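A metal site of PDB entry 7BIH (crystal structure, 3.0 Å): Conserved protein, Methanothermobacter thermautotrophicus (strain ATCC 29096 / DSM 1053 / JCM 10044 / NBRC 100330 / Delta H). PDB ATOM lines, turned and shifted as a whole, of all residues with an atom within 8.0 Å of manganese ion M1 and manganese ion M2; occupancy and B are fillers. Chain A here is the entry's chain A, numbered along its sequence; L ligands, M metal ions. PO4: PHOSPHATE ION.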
ATOM      1  N   SER A  42      -6.630 -22.368  31.870  1.00  0.00           N
ATOM      2  CA  SER A  42      -8.064 -22.522  31.730  1.00  0.00           C
ATOM      3  C   SER A  42      -8.849 -22.292  32.997  1.00  0.00           C
ATOM      4  O   SER A  42      -8.299 -22.064  34.075  1.00  0.00           O
ATOM      5  CB  SER A  42      -8.403 -23.897  31.150  1.00  0.00           C
ATOM      6  OG  SER A  42      -9.746 -23.959  30.682  1.00  0.00           O
ATOM      7  N   HIS A  43     -10.162 -22.348  32.815  1.00  0.00           N
ATOM      8  CA  HIS A  43     -11.143 -22.087  33.878  1.00  0.00           C
ATOM      9  C   HIS A  43     -11.449 -23.368  34.644  1.00  0.00           C
ATOM     10  O   HIS A  43     -11.008 -24.455  34.239  1.00  0.00           O
ATOM     11  CB  HIS A  43     -12.396 -21.506  33.241  1.00  0.00           C
ATOM     12  CG  HIS A  43     -13.287 -20.773  34.179  1.00  0.00           C
ATOM     13  ND1 HIS A  43     -14.631 -21.026  34.264  1.00  0.00           N
ATOM     14  CD2 HIS A  43     -13.021 -19.787  35.069  1.00  0.00           C
ATOM     15  CE1 HIS A  43     -15.168 -20.236  35.166  1.00  0.00           C
ATOM     16  NE2 HIS A  43     -14.215 -19.485  35.689  1.00  0.00           N
ATOM     17  N   ASN A  44     -12.199 -23.252  35.737  1.00  0.00           N
ATOM     18  CA  ASN A  44     -12.362 -24.322  36.736  1.00  0.00           C
ATOM     19  C   ASN A  44     -13.732 -24.968  36.827  1.00  0.00           C
ATOM     20  O   ASN A  44     -14.073 -25.553  37.845  1.00  0.00           O
ATOM     21  CB  ASN A  44     -12.002 -23.778  38.112  1.00  0.00           C
ATOM     22  CG  ASN A  44     -12.942 -22.700  38.573  1.00  0.00           C
ATOM     23  OD1 ASN A  44     -13.700 -22.115  37.786  1.00  0.00           O
ATOM     24  ND2 ASN A  44     -12.884 -22.408  39.840  1.00  0.00           N
ATOM     25  N   ASP A  45     -14.530 -24.852  35.769  1.00  0.00           N
ATOM     26  CA  ASP A  45     -15.842 -25.480  35.677  1.00  0.00           C
ATOM     27  C   ASP A  45     -15.803 -26.567  34.574  1.00  0.00           C
ATOM     28  O   ASP A  45     -14.759 -26.825  34.003  1.00  0.00           O
ATOM     29  CB  ASP A  45     -16.918 -24.415  35.433  1.00  0.00           C
ATOM     30  CG  ASP A  45     -16.621 -23.507  34.261  1.00  0.00           C
ATOM     31  OD1 ASP A  45     -15.744 -23.806  33.431  1.00  0.00           O
ATOM     32  OD2 ASP A  45     -17.239 -22.435  34.157  1.00  0.00           O
ATOM     33  N   ALA A  46     -16.931 -27.214  34.297  1.00  0.00           N
ATOM     34  CA  ALA A  46     -16.962 -28.285  33.308  1.00  0.00           C
ATOM     35  C   ALA A  46     -16.378 -27.838  31.993  1.00  0.00           C
ATOM     36  O   ALA A  46     -15.527 -28.529  31.428  1.00  0.00           O
ATOM     37  CB  ALA A  46     -18.386 -28.788  33.114  1.00  0.00           C
ATOM     38  N   ASP A  47     -16.836 -26.706  31.494  1.00  0.00           N
ATOM     39  CA  ASP A  47     -16.371 -26.171  30.215  1.00  0.00           C
ATOM     40  C   ASP A  47     -14.867 -25.903  30.249  1.00  0.00           C
ATOM     41  O   ASP A  47     -14.153 -26.275  29.329  1.00  0.00           O
ATOM     42  CB  ASP A  47     -17.125 -24.885  29.865  1.00  0.00           C
ATOM     43  CG  ASP A  47     -16.841 -24.389  28.476  1.00  0.00           C
ATOM     44  OD1 ASP A  47     -16.703 -25.224  27.561  1.00  0.00           O
ATOM     45  OD2 ASP A  47     -16.817 -23.134  28.278  1.00  0.00           O
ATOM     46  N   GLY A  48     -14.386 -25.298  31.312  1.00  0.00           N
ATOM     47  CA  GLY A  48     -12.987 -24.973  31.438  1.00  0.00           C
ATOM     48  C   GLY A  48     -12.084 -26.172  31.525  1.00  0.00           C
ATOM     49  O   GLY A  48     -11.028 -26.208  30.896  1.00  0.00           O
ATOM     50  N   LEU A  49     -12.503 -27.148  32.311  1.00  0.00           N
ATOM     51  CA  LEU A  49     -11.737 -28.378  32.447  1.00  0.00           C
ATOM     52  C   LEU A  49     -11.796 -29.266  31.188  1.00  0.00           C
ATOM     53  O   LEU A  49     -10.780 -29.837  30.792  1.00  0.00           O
ATOM     54  CB  LEU A  49     -12.179 -29.157  33.657  1.00  0.00           C
ATOM     55  CG  LEU A  49     -11.903 -28.536  35.009  1.00  0.00           C
ATOM     56  CD1 LEU A  49     -12.453 -29.477  36.068  1.00  0.00           C
ATOM     57  CD2 LEU A  49     -10.434 -28.374  35.283  1.00  0.00           C
ATOM     58  N   ALA A  51     -12.321 -28.144  28.117  1.00  0.00           N
ATOM     59  CA  ALA A  51     -11.502 -27.426  27.135  1.00  0.00           C
ATOM     60  C   ALA A  51     -10.012 -27.694  27.346  1.00  0.00           C
ATOM     61  O   ALA A  51      -9.303 -28.034  26.394  1.00  0.00           O
ATOM     62  CB  ALA A  51     -11.787 -25.923  27.159  1.00  0.00           C
ATOM     63  N   LEU A  71      -7.552 -21.683  36.747  1.00  0.00           N
ATOM     64  CA  LEU A  71      -7.894 -20.485  37.525  1.00  0.00           C
ATOM     65  C   LEU A  71      -9.396 -20.310  37.602  1.00  0.00           C
ATOM     66  O   LEU A  71     -10.101 -20.669  36.659  1.00  0.00           O
ATOM     67  CB  LEU A  71      -7.361 -19.245  36.815  1.00  0.00           C
ATOM     68  CG  LEU A  71      -5.883 -19.238  36.418  1.00  0.00           C
ATOM     69  CD1 LEU A  71      -5.618 -17.945  35.676  1.00  0.00           C
ATOM     70  CD2 LEU A  71      -4.965 -19.375  37.628  1.00  0.00           C
ATOM     71  N   SER A  72      -9.874 -19.725  38.697  1.00  0.00           N
ATOM     72  CA  SER A  72     -11.301 -19.360  38.837  1.00  0.00           C
ATOM     73  C   SER A  72     -11.632 -18.013  38.188  1.00  0.00           C
ATOM     74  O   SER A  72     -12.776 -17.754  37.852  1.00  0.00           O
ATOM     75  CB  SER A  72     -11.723 -19.340  40.289  1.00  0.00           C
ATOM     76  OG  SER A  72     -10.870 -18.518  41.029  1.00  0.00           O
ATOM     77  N   CYS A  93      -8.036 -20.991  27.501  1.00  0.00           N
ATOM     78  CA  CYS A  93      -9.388 -21.511  27.279  1.00  0.00           C
ATOM     79  C   CYS A  93     -10.403 -20.887  28.243  1.00  0.00           C
ATOM     80  O   CYS A  93     -10.150 -20.794  29.449  1.00  0.00           O
ATOM     81  CB  CYS A  93      -9.402 -23.026  27.484  1.00  0.00           C
ATOM     82  SG  CYS A  93      -8.157 -23.975  26.564  1.00  0.00           S
ATOM     83  N   ASP A  94     -11.546 -20.491  27.701  1.00  0.00           N
ATOM     84  CA  ASP A  94     -12.708 -20.018  28.504  1.00  0.00           C
ATOM     85  C   ASP A  94     -12.465 -18.688  29.209  1.00  0.00           C
ATOM     86  O   ASP A  94     -13.172 -18.346  30.148  1.00  0.00           O
ATOM     87  CB  ASP A  94     -13.107 -21.099  29.532  1.00  0.00           C
ATOM     88  CG  ASP A  94     -14.574 -21.023  29.956  1.00  0.00           C
ATOM     89  OD1 ASP A  94     -15.455 -20.517  29.198  1.00  0.00           O
ATOM     90  OD2 ASP A  94     -14.850 -21.511  31.066  1.00  0.00           O
ATOM     91  N   MET A  95     -11.466 -17.947  28.730  1.00  0.00           N
ATOM     92  CA  MET A  95     -11.089 -16.668  29.283  1.00  0.00           C
ATOM     93  C   MET A  95     -10.102 -16.004  28.354  1.00  0.00           C
ATOM     94  O   MET A  95      -9.637 -16.635  27.418  1.00  0.00           O
ATOM     95  CB  MET A  95     -10.484 -16.805  30.678  1.00  0.00           C
ATOM     96  CG  MET A  95      -9.243 -17.665  30.783  1.00  0.00           C
ATOM     97  SD  MET A  95      -9.123 -18.270  32.476  1.00  0.00           S
ATOM     98  CE  MET A  95      -7.471 -18.894  32.496  1.00  0.00           C
ATOM     99  N   ALA A 113      -8.871 -19.303  23.086  1.00  0.00           N
ATOM    100  CA  ALA A 113     -10.094 -20.004  22.768  1.00  0.00           C
ATOM    101  C   ALA A 113     -11.152 -19.622  23.797  1.00  0.00           C
ATOM    102  O   ALA A 113     -11.117 -20.063  24.937  1.00  0.00           O
ATOM    103  CB  ALA A 113      -9.839 -21.509  22.825  1.00  0.00           C
ATOM    104  N   ASP A 114     -12.101 -18.782  23.401  1.00  0.00           N
ATOM    105  CA  ASP A 114     -13.020 -18.213  24.373  1.00  0.00           C
ATOM    106  C   ASP A 114     -14.365 -17.903  23.734  1.00  0.00           C
ATOM    107  O   ASP A 114     -14.490 -17.958  22.501  1.00  0.00           O
ATOM    108  CB  ASP A 114     -12.394 -16.956  24.967  1.00  0.00           C
ATOM    109  CG  ASP A 114     -13.030 -16.540  26.285  1.00  0.00           C
ATOM    110  OD1 ASP A 114     -13.894 -17.288  26.804  1.00  0.00           O
ATOM    111  OD2 ASP A 114     -12.694 -15.430  26.754  1.00  0.00           O
ATOM    112  N   HIS A 115     -15.377 -17.641  24.554  1.00  0.00           N
ATOM    113  CA  HIS A 115     -16.714 -17.392  24.017  1.00  0.00           C
ATOM    114  C   HIS A 115     -17.501 -16.331  24.743  1.00  0.00           C
ATOM    115  O   HIS A 115     -18.723 -16.287  24.622  1.00  0.00           O
ATOM    116  CB  HIS A 115     -17.487 -18.714  23.905  1.00  0.00           C
ATOM    117  CG  HIS A 115     -17.889 -19.326  25.212  1.00  0.00           C
ATOM    118  ND1 HIS A 115     -19.205 -19.648  25.488  1.00  0.00           N
ATOM    119  CD2 HIS A 115     -17.168 -19.725  26.298  1.00  0.00           C
ATOM    120  CE1 HIS A 115     -19.270 -20.207  26.692  1.00  0.00           C
ATOM    121  NE2 HIS A 115     -18.049 -20.272  27.198  1.00  0.00           N
ATOM    122  N   HIS A 116     -16.796 -15.452  25.461  1.00  0.00           N
ATOM    123  CA  HIS A 116     -17.400 -14.271  26.055  1.00  0.00           C
ATOM    124  C   HIS A 116     -17.375 -13.118  25.039  1.00  0.00           C
ATOM    125  O   HIS A 116     -16.508 -13.089  24.167  1.00  0.00           O
ATOM    126  CB  HIS A 116     -16.637 -13.907  27.317  1.00  0.00           C
ATOM    127  CG  HIS A 116     -16.667 -14.963  28.366  1.00  0.00           C
ATOM    128  ND1 HIS A 116     -15.855 -16.071  28.321  1.00  0.00           N
ATOM    129  CD2 HIS A 116     -17.407 -15.098  29.495  1.00  0.00           C
ATOM    130  CE1 HIS A 116     -16.081 -16.840  29.369  1.00  0.00           C
ATOM    131  NE2 HIS A 116     -17.017 -16.260  30.102  1.00  0.00           N
ATOM    132  N   GLY A 139     -22.045 -16.922  21.440  1.00  0.00           N
ATOM    133  CA  GLY A 139     -21.283 -17.561  22.524  1.00  0.00           C
ATOM    134  C   GLY A 139     -22.092 -18.104  23.716  1.00  0.00           C
ATOM    135  O   GLY A 139     -21.597 -18.901  24.505  1.00  0.00           O
ATOM    136  N   LEU A 143     -21.603 -22.292  20.867  1.00  0.00           N
ATOM    137  CA  LEU A 143     -20.259 -22.795  21.123  1.00  0.00           C
ATOM    138  C   LEU A 143     -19.714 -22.356  22.499  1.00  0.00           C
ATOM    139  O   LEU A 143     -20.005 -21.258  22.977  1.00  0.00           O
ATOM    140  CB  LEU A 143     -19.305 -22.322  20.037  1.00  0.00           C
ATOM    141  CG  LEU A 143     -17.952 -22.987  19.922  1.00  0.00           C
ATOM    142  CD1 LEU A 143     -18.100 -24.456  19.566  1.00  0.00           C
ATOM    143  CD2 LEU A 143     -17.173 -22.258  18.841  1.00  0.00           C
ATOM    144  N   SER A 144     -18.962 -23.246  23.141  1.00  0.00           N
ATOM    145  CA  SER A 144     -18.374 -23.005  24.449  1.00  0.00           C
ATOM    146  C   SER A 144     -16.862 -23.094  24.297  1.00  0.00           C
ATOM    147  O   SER A 144     -16.376 -23.301  23.184  1.00  0.00           O
ATOM    148  CB  SER A 144     -18.899 -24.017  25.504  1.00  0.00           C
ATOM    149  OG  SER A 144     -18.474 -25.362  25.282  1.00  0.00           O
ATOM    150  N   ALA A 145     -16.116 -22.916  25.383  1.00  0.00           N
ATOM    151  CA  ALA A 145     -14.671 -22.988  25.331  1.00  0.00           C
ATOM    152  C   ALA A 145     -14.162 -24.349  24.832  1.00  0.00           C
ATOM    153  O   ALA A 145     -13.261 -24.415  23.983  1.00  0.00           O
ATOM    154  CB  ALA A 145     -14.069 -22.677  26.686  1.00  0.00           C
ATOM    155  N   SER A 146     -14.756 -25.414  25.345  1.00  0.00           N
ATOM    156  CA  SER A 146     -14.364 -26.766  24.973  1.00  0.00           C
ATOM    157  C   SER A 146     -14.512 -27.040  23.465  1.00  0.00           C
ATOM    158  O   SER A 146     -13.593 -27.581  22.857  1.00  0.00           O
ATOM    159  CB  SER A 146     -15.164 -27.787  25.793  1.00  0.00           C
ATOM    160  OG  SER A 146     -16.547 -27.596  25.601  1.00  0.00           O
ATOM    161  N   GLY A 167     -18.342 -29.854  27.762  1.00  0.00           N
ATOM    162  CA  GLY A 167     -18.315 -28.439  28.130  1.00  0.00           C
ATOM    163  C   GLY A 167     -19.554 -27.680  27.675  1.00  0.00           C
ATOM    164  O   GLY A 167     -20.049 -26.829  28.404  1.00  0.00           O
ATOM    165  N   ALA A 168     -20.040 -27.990  26.481  1.00  0.00           N
ATOM    166  CA  ALA A 168     -21.238 -27.325  25.985  1.00  0.00           C
ATOM    167  C   ALA A 168     -22.396 -27.569  26.904  1.00  0.00           C
ATOM    168  O   ALA A 168     -23.150 -26.645  27.237  1.00  0.00           O
ATOM    169  CB  ALA A 168     -21.587 -27.773  24.564  1.00  0.00           C
ATOM    170  N   GLY A 170     -22.199 -28.592  30.069  1.00  0.00           N
ATOM    171  CA  GLY A 170     -21.789 -27.843  31.268  1.00  0.00           C
ATOM    172  C   GLY A 170     -22.174 -26.379  31.252  1.00  0.00           C
ATOM    173  O   GLY A 170     -22.706 -25.878  32.206  1.00  0.00           O
ATOM    174  N   ASP A 171     -21.967 -25.726  30.115  1.00  0.00           N
ATOM    175  CA  ASP A 171     -22.337 -24.316  29.936  1.00  0.00           C
ATOM    176  C   ASP A 171     -23.807 -24.114  29.446  1.00  0.00           C
ATOM    177  O   ASP A 171     -24.170 -23.026  29.020  1.00  0.00           O
ATOM    178  CB  ASP A 171     -21.348 -23.634  28.945  1.00  0.00           C
ATOM    179  CG  ASP A 171     -20.162 -22.991  29.632  1.00  0.00           C
ATOM    180  OD1 ASP A 171     -19.921 -23.288  30.840  1.00  0.00           O
ATOM    181  OD2 ASP A 171     -19.466 -22.186  28.958  1.00  0.00           O
ATOM    182  N   GLN A 173     -25.762 -25.157  26.930  1.00  0.00           N
ATOM    183  CA  GLN A 173     -25.963 -24.781  25.536  1.00  0.00           C
ATOM    184  C   GLN A 173     -26.853 -25.775  24.763  1.00  0.00           C
ATOM    185  O   GLN A 173     -27.034 -25.648  23.551  1.00  0.00           O
ATOM    186  CB  GLN A 173     -24.604 -24.579  24.843  1.00  0.00           C
ATOM    187  CG  GLN A 173     -23.791 -23.465  25.461  1.00  0.00           C
ATOM    188  CD  GLN A 173     -22.597 -23.011  24.637  1.00  0.00           C
ATOM    189  OE1 GLN A 173     -22.162 -23.711  23.717  1.00  0.00           O
ATOM    190  NE2 GLN A 173     -22.040 -21.839  24.995  1.00  0.00           N
ATOM    191  N   ASP A 294     -17.833 -30.592  37.122  1.00  0.00           N
ATOM    192  CA  ASP A 294     -18.276 -29.480  38.004  1.00  0.00           C
ATOM    193  C   ASP A 294     -17.933 -29.767  39.444  1.00  0.00           C
ATOM    194  O   ASP A 294     -17.507 -28.853  40.154  1.00  0.00           O
ATOM    195  CB  ASP A 294     -19.764 -29.189  37.874  1.00  0.00           C
ATOM    196  CG  ASP A 294     -20.102 -28.444  36.584  1.00  0.00           C
ATOM    197  OD1 ASP A 294     -19.372 -27.485  36.229  1.00  0.00           O
ATOM    198  OD2 ASP A 294     -21.118 -28.805  35.926  1.00  0.00           O
ATOM    199  N   HIS A 427     -22.101 -13.768  30.588  1.00  0.00           N
ATOM    200  CA  HIS A 427     -22.893 -13.904  29.371  1.00  0.00           C
ATOM    201  C   HIS A 427     -24.263 -13.269  29.645  1.00  0.00           C
ATOM    202  O   HIS A 427     -24.544 -12.806  30.761  1.00  0.00           O
ATOM    203  CB  HIS A 427     -23.067 -15.388  28.981  1.00  0.00           C
ATOM    204  CG  HIS A 427     -21.786 -16.156  28.829  1.00  0.00           C
ATOM    205  ND1 HIS A 427     -21.124 -16.302  27.626  1.00  0.00           N
ATOM    206  CD2 HIS A 427     -21.074 -16.881  29.722  1.00  0.00           C
ATOM    207  CE1 HIS A 427     -20.029 -17.028  27.791  1.00  0.00           C
ATOM    208  NE2 HIS A 427     -19.989 -17.401  29.054  1.00  0.00           N
HETATM  209  P   PO4 L   1     -18.301 -19.242  31.703  1.00  0.00           P
HETATM  210  O1  PO4 L   1     -17.081 -19.446  32.639  1.00  0.00           O
HETATM  211  O2  PO4 L   1     -18.401 -17.813  31.284  1.00  0.00           O
HETATM  212  O3  PO4 L   1     -19.619 -19.562  32.359  1.00  0.00           O
HETATM  213  O4  PO4 L   1     -18.178 -20.127  30.492  1.00  0.00           O
HETATM  214 MN    MN M   1     -17.376 -21.396  29.377  1.00  0.00          MN
HETATM  215 MN    MN M   2     -16.411 -21.458  32.264  1.00  0.00          MN
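Of the 30 residues printed, 4 come within 4 Å of manganese ion M1.
The nearest printed residue that does not touch manganese ion M1 is Ala 145 (4.5 Å).
Manganese ion M1 is bound by an oxygen (O4) of the ligand, the side-chain carboxylate of Asp 94, the side-chain carboxylate of Asp 47, the side-chain carboxylate of Asp 171 and a ring nitrogen (NE2) of His 115.
Manganese ion M1 has five donor atoms within binding distance.
Within 4 Å of manganese ion M2: His 43, Asp 45 and Asp 94.
The nearest printed residue that does not touch manganese ion M2 is Asp 171 (4.2 Å).
The side-chain carboxylate (OD1) of Asp 45 sits at hydrogen-bond distance from a ring nitrogen (ND1) of His 43.
NE2 of His 43 lies within hydrogen-bond range of OD1 of Asn 44, 3.4 Å away.
The side-chain carboxylate (OD1) of Asp 47 lies within hydrogen-bond range of the backbone NH (N) of Ser 146 (3.0 Å).
The backbone carbonyl oxygen (O) of Leu 143 sits at hydrogen-bond distance from a ring nitrogen (ND1) of His 115.
The side-chain carboxylate of Asp 94 lies close to a ring nitrogen (ND1) of His 43 (3.2 Å).
The backbone carbonyl oxygen of Ala 113 lies within hydrogen-bond range of the backbone NH of Asp 94, 2.8 Å away.
The backbone NH (N) of Gly 48 is in hydrogen-bond range of the side-chain carboxylate (OD1) of Asp 45, at 2.9 Å.
A ring nitrogen (ND1) of His 115 is in hydrogen-bond range of the backbone carbonyl oxygen of Gly 139.
Manganese ion M2 is bound by the side-chain carboxylate of Asp 94 (2.0 Å), an oxygen (O1) of the ligand (2.2 Å) and the side-chain carboxylate of Asp 45 (2.3 Å).
Slightly farther from manganese ion M2 lies the side-chain carboxylate (OD1) of Asp 45 (2.7 Å).
Slightly farther from manganese ion M2 lies ND1 of His 43 (2.7 Å).
Slightly farther from manganese ion M2 lies an oxygen (O4) of the ligand (2.8 Å).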
